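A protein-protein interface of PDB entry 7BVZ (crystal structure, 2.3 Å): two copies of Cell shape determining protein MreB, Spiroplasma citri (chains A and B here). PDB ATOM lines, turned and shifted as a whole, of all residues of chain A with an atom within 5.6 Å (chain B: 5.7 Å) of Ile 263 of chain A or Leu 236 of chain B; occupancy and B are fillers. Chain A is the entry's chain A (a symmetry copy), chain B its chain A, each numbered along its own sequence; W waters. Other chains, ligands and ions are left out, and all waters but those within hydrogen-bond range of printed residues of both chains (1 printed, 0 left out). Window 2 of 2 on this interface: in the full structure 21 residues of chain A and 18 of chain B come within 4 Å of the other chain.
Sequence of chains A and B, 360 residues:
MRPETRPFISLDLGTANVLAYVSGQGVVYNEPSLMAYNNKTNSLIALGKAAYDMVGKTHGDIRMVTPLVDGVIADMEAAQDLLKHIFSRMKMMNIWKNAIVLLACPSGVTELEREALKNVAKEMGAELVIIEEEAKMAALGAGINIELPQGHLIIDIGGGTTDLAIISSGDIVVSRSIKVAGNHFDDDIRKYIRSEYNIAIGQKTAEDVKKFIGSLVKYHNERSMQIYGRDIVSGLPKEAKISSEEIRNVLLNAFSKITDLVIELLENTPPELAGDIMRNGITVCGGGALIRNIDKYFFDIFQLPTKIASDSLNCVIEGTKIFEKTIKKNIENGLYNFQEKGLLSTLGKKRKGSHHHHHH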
ATOM      1  N   ILE A 258      23.013  -7.082 -36.626  1.00  0.00           N
ATOM      2  CA  ILE A 258      21.610  -7.302 -36.294  1.00  0.00           C
ATOM      3  C   ILE A 258      21.457  -8.494 -35.355  1.00  0.00           C
ATOM      4  O   ILE A 258      20.595  -8.484 -34.468  1.00  0.00           O
ATOM      5  CB  ILE A 258      20.782  -7.485 -37.578  1.00  0.00           C
ATOM      6  CG1 ILE A 258      20.858  -6.228 -38.447  1.00  0.00           C
ATOM      7  CG2 ILE A 258      19.330  -7.814 -37.248  1.00  0.00           C
ATOM      8  CD1 ILE A 258      20.037  -6.312 -39.718  1.00  0.00           C
ATOM      9  N   THR A 259      22.294  -9.521 -35.517  1.00  0.00           N
ATOM     10  CA  THR A 259      22.183 -10.720 -34.691  1.00  0.00           C
ATOM     11  C   THR A 259      22.519 -10.424 -33.234  1.00  0.00           C
ATOM     12  O   THR A 259      21.809 -10.863 -32.321  1.00  0.00           O
ATOM     13  CB  THR A 259      23.094 -11.818 -35.242  1.00  0.00           C
ATOM     14  OG1 THR A 259      22.680 -12.162 -36.569  1.00  0.00           O
ATOM     15  CG2 THR A 259      23.038 -13.056 -34.360  1.00  0.00           C
ATOM     16  N   ASP A 260      23.604  -9.681 -32.995  1.00  0.00           N
ATOM     17  CA  ASP A 260      23.989  -9.362 -31.625  1.00  0.00           C
ATOM     18  C   ASP A 260      22.971  -8.452 -30.953  1.00  0.00           C
ATOM     19  O   ASP A 260      22.836  -8.477 -29.724  1.00  0.00           O
ATOM     20  CB  ASP A 260      25.373  -8.717 -31.600  1.00  0.00           C
ATOM     21  CG  ASP A 260      26.445  -9.614 -32.184  1.00  0.00           C
ATOM     22  OD1 ASP A 260      26.255 -10.850 -32.184  1.00  0.00           O
ATOM     23  OD2 ASP A 260      27.477  -9.084 -32.643  1.00  0.00           O
ATOM     24  N   LEU A 261      22.253  -7.642 -31.732  1.00  0.00           N
ATOM     25  CA  LEU A 261      21.175  -6.841 -31.162  1.00  0.00           C
ATOM     26  C   LEU A 261      20.057  -7.732 -30.637  1.00  0.00           C
ATOM     27  O   LEU A 261      19.472  -7.449 -29.585  1.00  0.00           O
ATOM     28  CB  LEU A 261      20.639  -5.860 -32.203  1.00  0.00           C
ATOM     29  CG  LEU A 261      19.659  -4.807 -31.684  1.00  0.00           C
ATOM     30  CD1 LEU A 261      20.399  -3.722 -30.915  1.00  0.00           C
ATOM     31  CD2 LEU A 261      18.842  -4.211 -32.819  1.00  0.00           C
ATOM     32  N   VAL A 262      19.749  -8.814 -31.357  1.00  0.00           N
ATOM     33  CA  VAL A 262      18.777  -9.786 -30.862  1.00  0.00           C
ATOM     34  C   VAL A 262      19.270 -10.408 -29.563  1.00  0.00           C
ATOM     35  O   VAL A 262      18.497 -10.601 -28.617  1.00  0.00           O
ATOM     36  CB  VAL A 262      18.495 -10.859 -31.929  1.00  0.00           C
ATOM     37  CG1 VAL A 262      17.358 -11.767 -31.485  1.00  0.00           C
ATOM     38  CG2 VAL A 262      18.182 -10.220 -33.272  1.00  0.00           C
ATOM     39  N   ILE A 263      20.564 -10.732 -29.498  1.00  0.00           N
ATOM     40  CA  ILE A 263      21.141 -11.246 -28.260  1.00  0.00           C
ATOM     41  C   ILE A 263      20.986 -10.223 -27.142  1.00  0.00           C
ATOM     42  O   ILE A 263      20.694 -10.575 -25.994  1.00  0.00           O
ATOM     43  CB  ILE A 263      22.618 -11.627 -28.473  1.00  0.00           C
ATOM     44  CG1 ILE A 263      22.760 -12.610 -29.636  1.00  0.00           C
ATOM     45  CG2 ILE A 263      23.205 -12.220 -27.203  1.00  0.00           C
ATOM     46  CD1 ILE A 263      22.250 -13.999 -29.332  1.00  0.00           C
ATOM     47  N   GLU A 264      21.167  -8.940 -27.464  1.00  0.00           N
ATOM     48  CA  GLU A 264      21.034  -7.899 -26.451  1.00  0.00           C
ATOM     49  C   GLU A 264      19.577  -7.699 -26.052  1.00  0.00           C
ATOM     50  O   GLU A 264      19.279  -7.425 -24.884  1.00  0.00           O
ATOM     51  CB  GLU A 264      21.642  -6.591 -26.959  1.00  0.00           C
ATOM     52  CG  GLU A 264      21.765  -5.514 -25.895  1.00  0.00           C
ATOM     53  CD  GLU A 264      22.287  -4.203 -26.447  1.00  0.00           C
ATOM     54  OE1 GLU A 264      23.066  -4.231 -27.423  1.00  0.00           O
ATOM     55  OE2 GLU A 264      21.911  -3.142 -25.905  1.00  0.00           O
ATOM     56  N   LEU A 265      18.654  -7.825 -27.011  1.00  0.00           N
ATOM     57  CA  LEU A 265      17.234  -7.722 -26.686  1.00  0.00           C
ATOM     58  C   LEU A 265      16.790  -8.876 -25.797  1.00  0.00           C
ATOM     59  O   LEU A 265      16.027  -8.676 -24.844  1.00  0.00           O
ATOM     60  CB  LEU A 265      16.402  -7.682 -27.967  1.00  0.00           C
ATOM     61  CG  LEU A 265      14.890  -7.506 -27.800  1.00  0.00           C
ATOM     62  CD1 LEU A 265      14.533  -6.040 -27.614  1.00  0.00           C
ATOM     63  CD2 LEU A 265      14.137  -8.100 -28.980  1.00  0.00           C
ATOM     64  N   LEU A 266      17.258 -10.091 -26.090  1.00  0.00           N
ATOM     65  CA  LEU A 266      16.935 -11.237 -25.249  1.00  0.00           C
ATOM     66  C   LEU A 266      17.706 -11.227 -23.936  1.00  0.00           C
ATOM     67  O   LEU A 266      17.259 -11.853 -22.968  1.00  0.00           O
ATOM     68  CB  LEU A 266      17.205 -12.542 -25.999  1.00  0.00           C
ATOM     69  CG  LEU A 266      16.074 -13.092 -26.874  1.00  0.00           C
ATOM     70  CD1 LEU A 266      14.773 -13.155 -26.089  1.00  0.00           C
ATOM     71  CD2 LEU A 266      15.899 -12.274 -28.138  1.00  0.00           C
ATOM     72  N   GLU A 267      18.848 -10.537 -23.879  1.00  0.00           N
ATOM     73  CA  GLU A 267      19.599 -10.455 -22.628  1.00  0.00           C
ATOM     74  C   GLU A 267      18.809  -9.716 -21.556  1.00  0.00           C
ATOM     75  O   GLU A 267      18.838 -10.097 -20.381  1.00  0.00           O
ATOM     76  CB  GLU A 267      20.943  -9.765 -22.860  1.00  0.00           C
ATOM     77  CG  GLU A 267      22.099 -10.711 -23.139  1.00  0.00           C
ATOM     78  CD  GLU A 267      23.419  -9.983 -23.291  1.00  0.00           C
ATOM     79  OE1 GLU A 267      23.449  -8.751 -23.083  1.00  0.00           O
ATOM     80  OE2 GLU A 267      24.429 -10.642 -23.619  1.00  0.00           O
ATOM     81  N   ASN A 268      18.098  -8.656 -21.940  1.00  0.00           N
ATOM     82  CA  ASN A 268      17.351  -7.829 -21.004  1.00  0.00           C
ATOM     83  C   ASN A 268      15.855  -8.119 -21.035  1.00  0.00           C
ATOM     84  O   ASN A 268      15.055  -7.268 -20.632  1.00  0.00           O
ATOM     85  CB  ASN A 268      17.616  -6.350 -21.288  1.00  0.00           C
ATOM     86  CG  ASN A 268      19.080  -5.989 -21.155  1.00  0.00           C
ATOM     87  OD1 ASN A 268      19.842  -6.066 -22.120  1.00  0.00           O
ATOM     88  ND2 ASN A 268      19.486  -5.600 -19.952  1.00  0.00           N
ATOM     89  N   ILE A 301      20.434 -19.793 -35.706  1.00  0.00           N
ATOM     90  CA  ILE A 301      21.276 -19.049 -34.774  1.00  0.00           C
ATOM     91  C   ILE A 301      20.720 -19.098 -33.358  1.00  0.00           C
ATOM     92  O   ILE A 301      21.434 -19.441 -32.411  1.00  0.00           O
ATOM     93  CB  ILE A 301      21.444 -17.593 -35.257  1.00  0.00           C
ATOM     94  CG1 ILE A 301      22.178 -17.554 -36.598  1.00  0.00           C
ATOM     95  CG2 ILE A 301      22.188 -16.768 -34.219  1.00  0.00           C
ATOM     96  CD1 ILE A 301      22.441 -16.157 -37.094  1.00  0.00           C
ATOM     97  N   PHE A 302      19.445 -18.757 -33.185  1.00  0.00           N
ATOM     98  CA  PHE A 302      18.852 -18.613 -31.863  1.00  0.00           C
ATOM     99  C   PHE A 302      18.067 -19.837 -31.412  1.00  0.00           C
ATOM    100  O   PHE A 302      17.561 -19.841 -30.285  1.00  0.00           O
ATOM    101  CB  PHE A 302      17.932 -17.389 -31.827  1.00  0.00           C
ATOM    102  CG  PHE A 302      18.552 -16.141 -32.382  1.00  0.00           C
ATOM    103  CD1 PHE A 302      19.522 -15.455 -31.670  1.00  0.00           C
ATOM    104  CD2 PHE A 302      18.151 -15.644 -33.610  1.00  0.00           C
ATOM    105  CE1 PHE A 302      20.089 -14.303 -32.179  1.00  0.00           C
ATOM    106  CE2 PHE A 302      18.714 -14.492 -34.126  1.00  0.00           C
ATOM    107  CZ  PHE A 302      19.684 -13.822 -33.410  1.00  0.00           C
ATOM    108  N   LEU A 304      15.236 -20.511 -32.258  1.00  0.00           N
ATOM    109  CA  LEU A 304      13.896 -19.981 -32.065  1.00  0.00           C
ATOM    110  C   LEU A 304      13.077 -20.166 -33.330  1.00  0.00           C
ATOM    111  O   LEU A 304      13.569 -19.863 -34.426  1.00  0.00           O
ATOM    112  CB  LEU A 304      13.949 -18.493 -31.697  1.00  0.00           C
ATOM    113  CG  LEU A 304      14.567 -18.109 -30.351  1.00  0.00           C
ATOM    114  CD1 LEU A 304      14.729 -16.603 -30.254  1.00  0.00           C
ATOM    115  CD2 LEU A 304      13.716 -18.627 -29.209  1.00  0.00           C
ATOM    116  N   GLY B 229      12.642 -20.544 -19.879  1.00  0.00           N
ATOM    117  CA  GLY B 229      13.098 -19.330 -19.232  1.00  0.00           C
ATOM    118  C   GLY B 229      14.277 -18.689 -19.931  1.00  0.00           C
ATOM    119  O   GLY B 229      14.518 -18.948 -21.114  1.00  0.00           O
ATOM    120  N   ARG B 230      15.021 -17.852 -19.214  1.00  0.00           N
ATOM    121  CA  ARG B 230      16.178 -17.157 -19.763  1.00  0.00           C
ATOM    122  C   ARG B 230      17.455 -17.813 -19.258  1.00  0.00           C
ATOM    123  O   ARG B 230      17.614 -18.028 -18.052  1.00  0.00           O
ATOM    124  CB  ARG B 230      16.162 -15.677 -19.381  1.00  0.00           C
ATOM    125  CG  ARG B 230      17.325 -14.883 -19.951  1.00  0.00           C
ATOM    126  CD  ARG B 230      17.871 -13.889 -18.941  1.00  0.00           C
ATOM    127  NE  ARG B 230      16.881 -12.889 -18.556  1.00  0.00           N
ATOM    128  CZ  ARG B 230      17.068 -11.982 -17.604  1.00  0.00           C
ATOM    129  NH1 ARG B 230      16.111 -11.107 -17.319  1.00  0.00           N
ATOM    130  NH2 ARG B 230      18.211 -11.949 -16.934  1.00  0.00           N
ATOM    131  N   ASP B 231      18.361 -18.124 -20.179  1.00  0.00           N
ATOM    132  CA  ASP B 231      19.631 -18.740 -19.817  1.00  0.00           C
ATOM    133  C   ASP B 231      20.565 -17.693 -19.222  1.00  0.00           C
ATOM    134  O   ASP B 231      20.749 -16.614 -19.793  1.00  0.00           O
ATOM    135  CB  ASP B 231      20.266 -19.399 -21.042  1.00  0.00           C
ATOM    136  CG  ASP B 231      21.577 -20.096 -20.725  1.00  0.00           C
ATOM    137  OD1 ASP B 231      21.882 -20.306 -19.533  1.00  0.00           O
ATOM    138  OD2 ASP B 231      22.301 -20.446 -21.678  1.00  0.00           O
ATOM    139  N   SER B 234      24.038 -17.859 -21.831  1.00  0.00           N
ATOM    140  CA  SER B 234      23.921 -17.340 -23.188  1.00  0.00           C
ATOM    141  C   SER B 234      23.075 -16.077 -23.279  1.00  0.00           C
ATOM    142  O   SER B 234      23.232 -15.314 -24.238  1.00  0.00           O
ATOM    143  CB  SER B 234      23.330 -18.406 -24.112  1.00  0.00           C
ATOM    144  OG  SER B 234      21.969 -18.654 -23.798  1.00  0.00           O
ATOM    145  N   GLY B 235      22.187 -15.839 -22.313  1.00  0.00           N
ATOM    146  CA  GLY B 235      21.242 -14.747 -22.399  1.00  0.00           C
ATOM    147  C   GLY B 235      20.033 -15.022 -23.263  1.00  0.00           C
ATOM    148  O   GLY B 235      19.063 -14.254 -23.205  1.00  0.00           O
ATOM    149  N   LEU B 236      20.055 -16.084 -24.062  1.00  0.00           N
ATOM    150  CA  LEU B 236      18.962 -16.498 -24.924  1.00  0.00           C
ATOM    151  C   LEU B 236      17.984 -17.379 -24.160  1.00  0.00           C
ATOM    152  O   LEU B 236      18.339 -17.985 -23.145  1.00  0.00           O
ATOM    153  CB  LEU B 236      19.510 -17.255 -26.133  1.00  0.00           C
ATOM    154  CG  LEU B 236      20.254 -16.432 -27.182  1.00  0.00           C
ATOM    155  CD1 LEU B 236      20.925 -17.347 -28.194  1.00  0.00           C
ATOM    156  CD2 LEU B 236      19.295 -15.479 -27.875  1.00  0.00           C
ATOM    157  N   PRO B 237      16.733 -17.460 -24.616  1.00  0.00           N
ATOM    158  CA  PRO B 237      15.776 -18.367 -23.972  1.00  0.00           C
ATOM    159  C   PRO B 237      16.239 -19.814 -24.064  1.00  0.00           C
ATOM    160  O   PRO B 237      16.715 -20.269 -25.106  1.00  0.00           O
ATOM    161  CB  PRO B 237      14.483 -18.136 -24.761  1.00  0.00           C
ATOM    162  CG  PRO B 237      14.633 -16.774 -25.345  1.00  0.00           C
ATOM    163  CD  PRO B 237      16.094 -16.630 -25.651  1.00  0.00           C
ATOM    164  N   LYS B 238      16.096 -20.539 -22.955  1.00  0.00           N
ATOM    165  CA  LYS B 238      16.570 -21.913 -22.860  1.00  0.00           C
ATOM    166  C   LYS B 238      15.490 -22.800 -22.256  1.00  0.00           C
ATOM    167  O   LYS B 238      14.732 -22.367 -21.382  1.00  0.00           O
ATOM    168  CB  LYS B 238      17.854 -22.000 -22.022  1.00  0.00           C
ATOM    169  CG  LYS B 238      18.569 -23.339 -22.120  1.00  0.00           C
ATOM    170  CD  LYS B 238      19.911 -23.311 -21.410  1.00  0.00           C
ATOM    171  CE  LYS B 238      20.651 -24.628 -21.594  1.00  0.00           C
ATOM    172  NZ  LYS B 238      22.014 -24.596 -20.995  1.00  0.00           N
HETATM  173  O   HOH W   1      16.315 -14.263 -23.322  1.00  0.00           O
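O of Gly 235 of chain B sits close to O of Leu 266 of chain A, 3.0 Å away.
The backbone carbonyl oxygen (O) of Leu 236 of chain B lies within hydrogen-bond range of the backbone NH (N) of Asp 231 of chain B, at 3.0 Å.
OG of Ser 234 of chain B sits close to N of Leu 236 of chain B (3.2 Å).
CD1 of Ile 263 of chain A touches CD2 of Leu 236 of chain B, at 3.6 Å.
Pro 237 of chain B touches Leu 266 of chain A (CG to CD1, 3.7 Å).
Glu 267 of chain A touches Arg 230 of chain B.
Glu 267 of chain A touches Gly 235 of chain B (N to O, 3.8 Å).
Phe 302 of chain A touches Leu 236 of chain B (CD1 to CD2, 3.8 Å).
Printed residues of chain B within 4 Å of Ile 263 of chain A: Leu 236 (3.6 Å).
Of chain A, only Ile 263 and Phe 302 come within 4 Å of Leu 236 of chain B.
Of the printed residues of chain B, Phe 302 of chain A touches Leu 236.
Of the printed residues of chain A, Arg 230 of chain B touches Glu 267 (3.8 Å).
Of the printed residues of chain A, Pro 237 of chain B touches Leu 266.
Of the printed residues of chain B, Leu 266 of chain A touches Gly 235 and Pro 237.
Ser 234 of chain B touches none of the printed residues of chain A.
The nearest residue of chain A that does not touch Leu 236 of chain B is Leu 266 of chain A (4.1 Å).
The nearest printed residue of chain B that does not touch Leu 266 of chain A is Leu 236 of chain B (4.1 Å).
Of the 14 printed residues of chain A, 4 touch a printed residue of chain B.
Hydrophobic or aromatic side chains of chain A within 4 Å of the printed part of chain B: Ile 263, Leu 266 and Phe 302.
Of the 8 printed residues of chain B, 4 touch a printed residue of chain A.
Hydrophobic or aromatic side chains of chain B that line the printed part of chain A: Leu 236 and Pro 237.
Among the printed residues, no Asp or Glu carboxylate lies within 4 Å of a Lys or Arg side-chain nitrogen of the other chain.
No position is printed for both chains.
Water W1 bridges O of Leu 266 of chain A (2.6 Å) and O of Gly 235 of chain B (2.8 Å).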
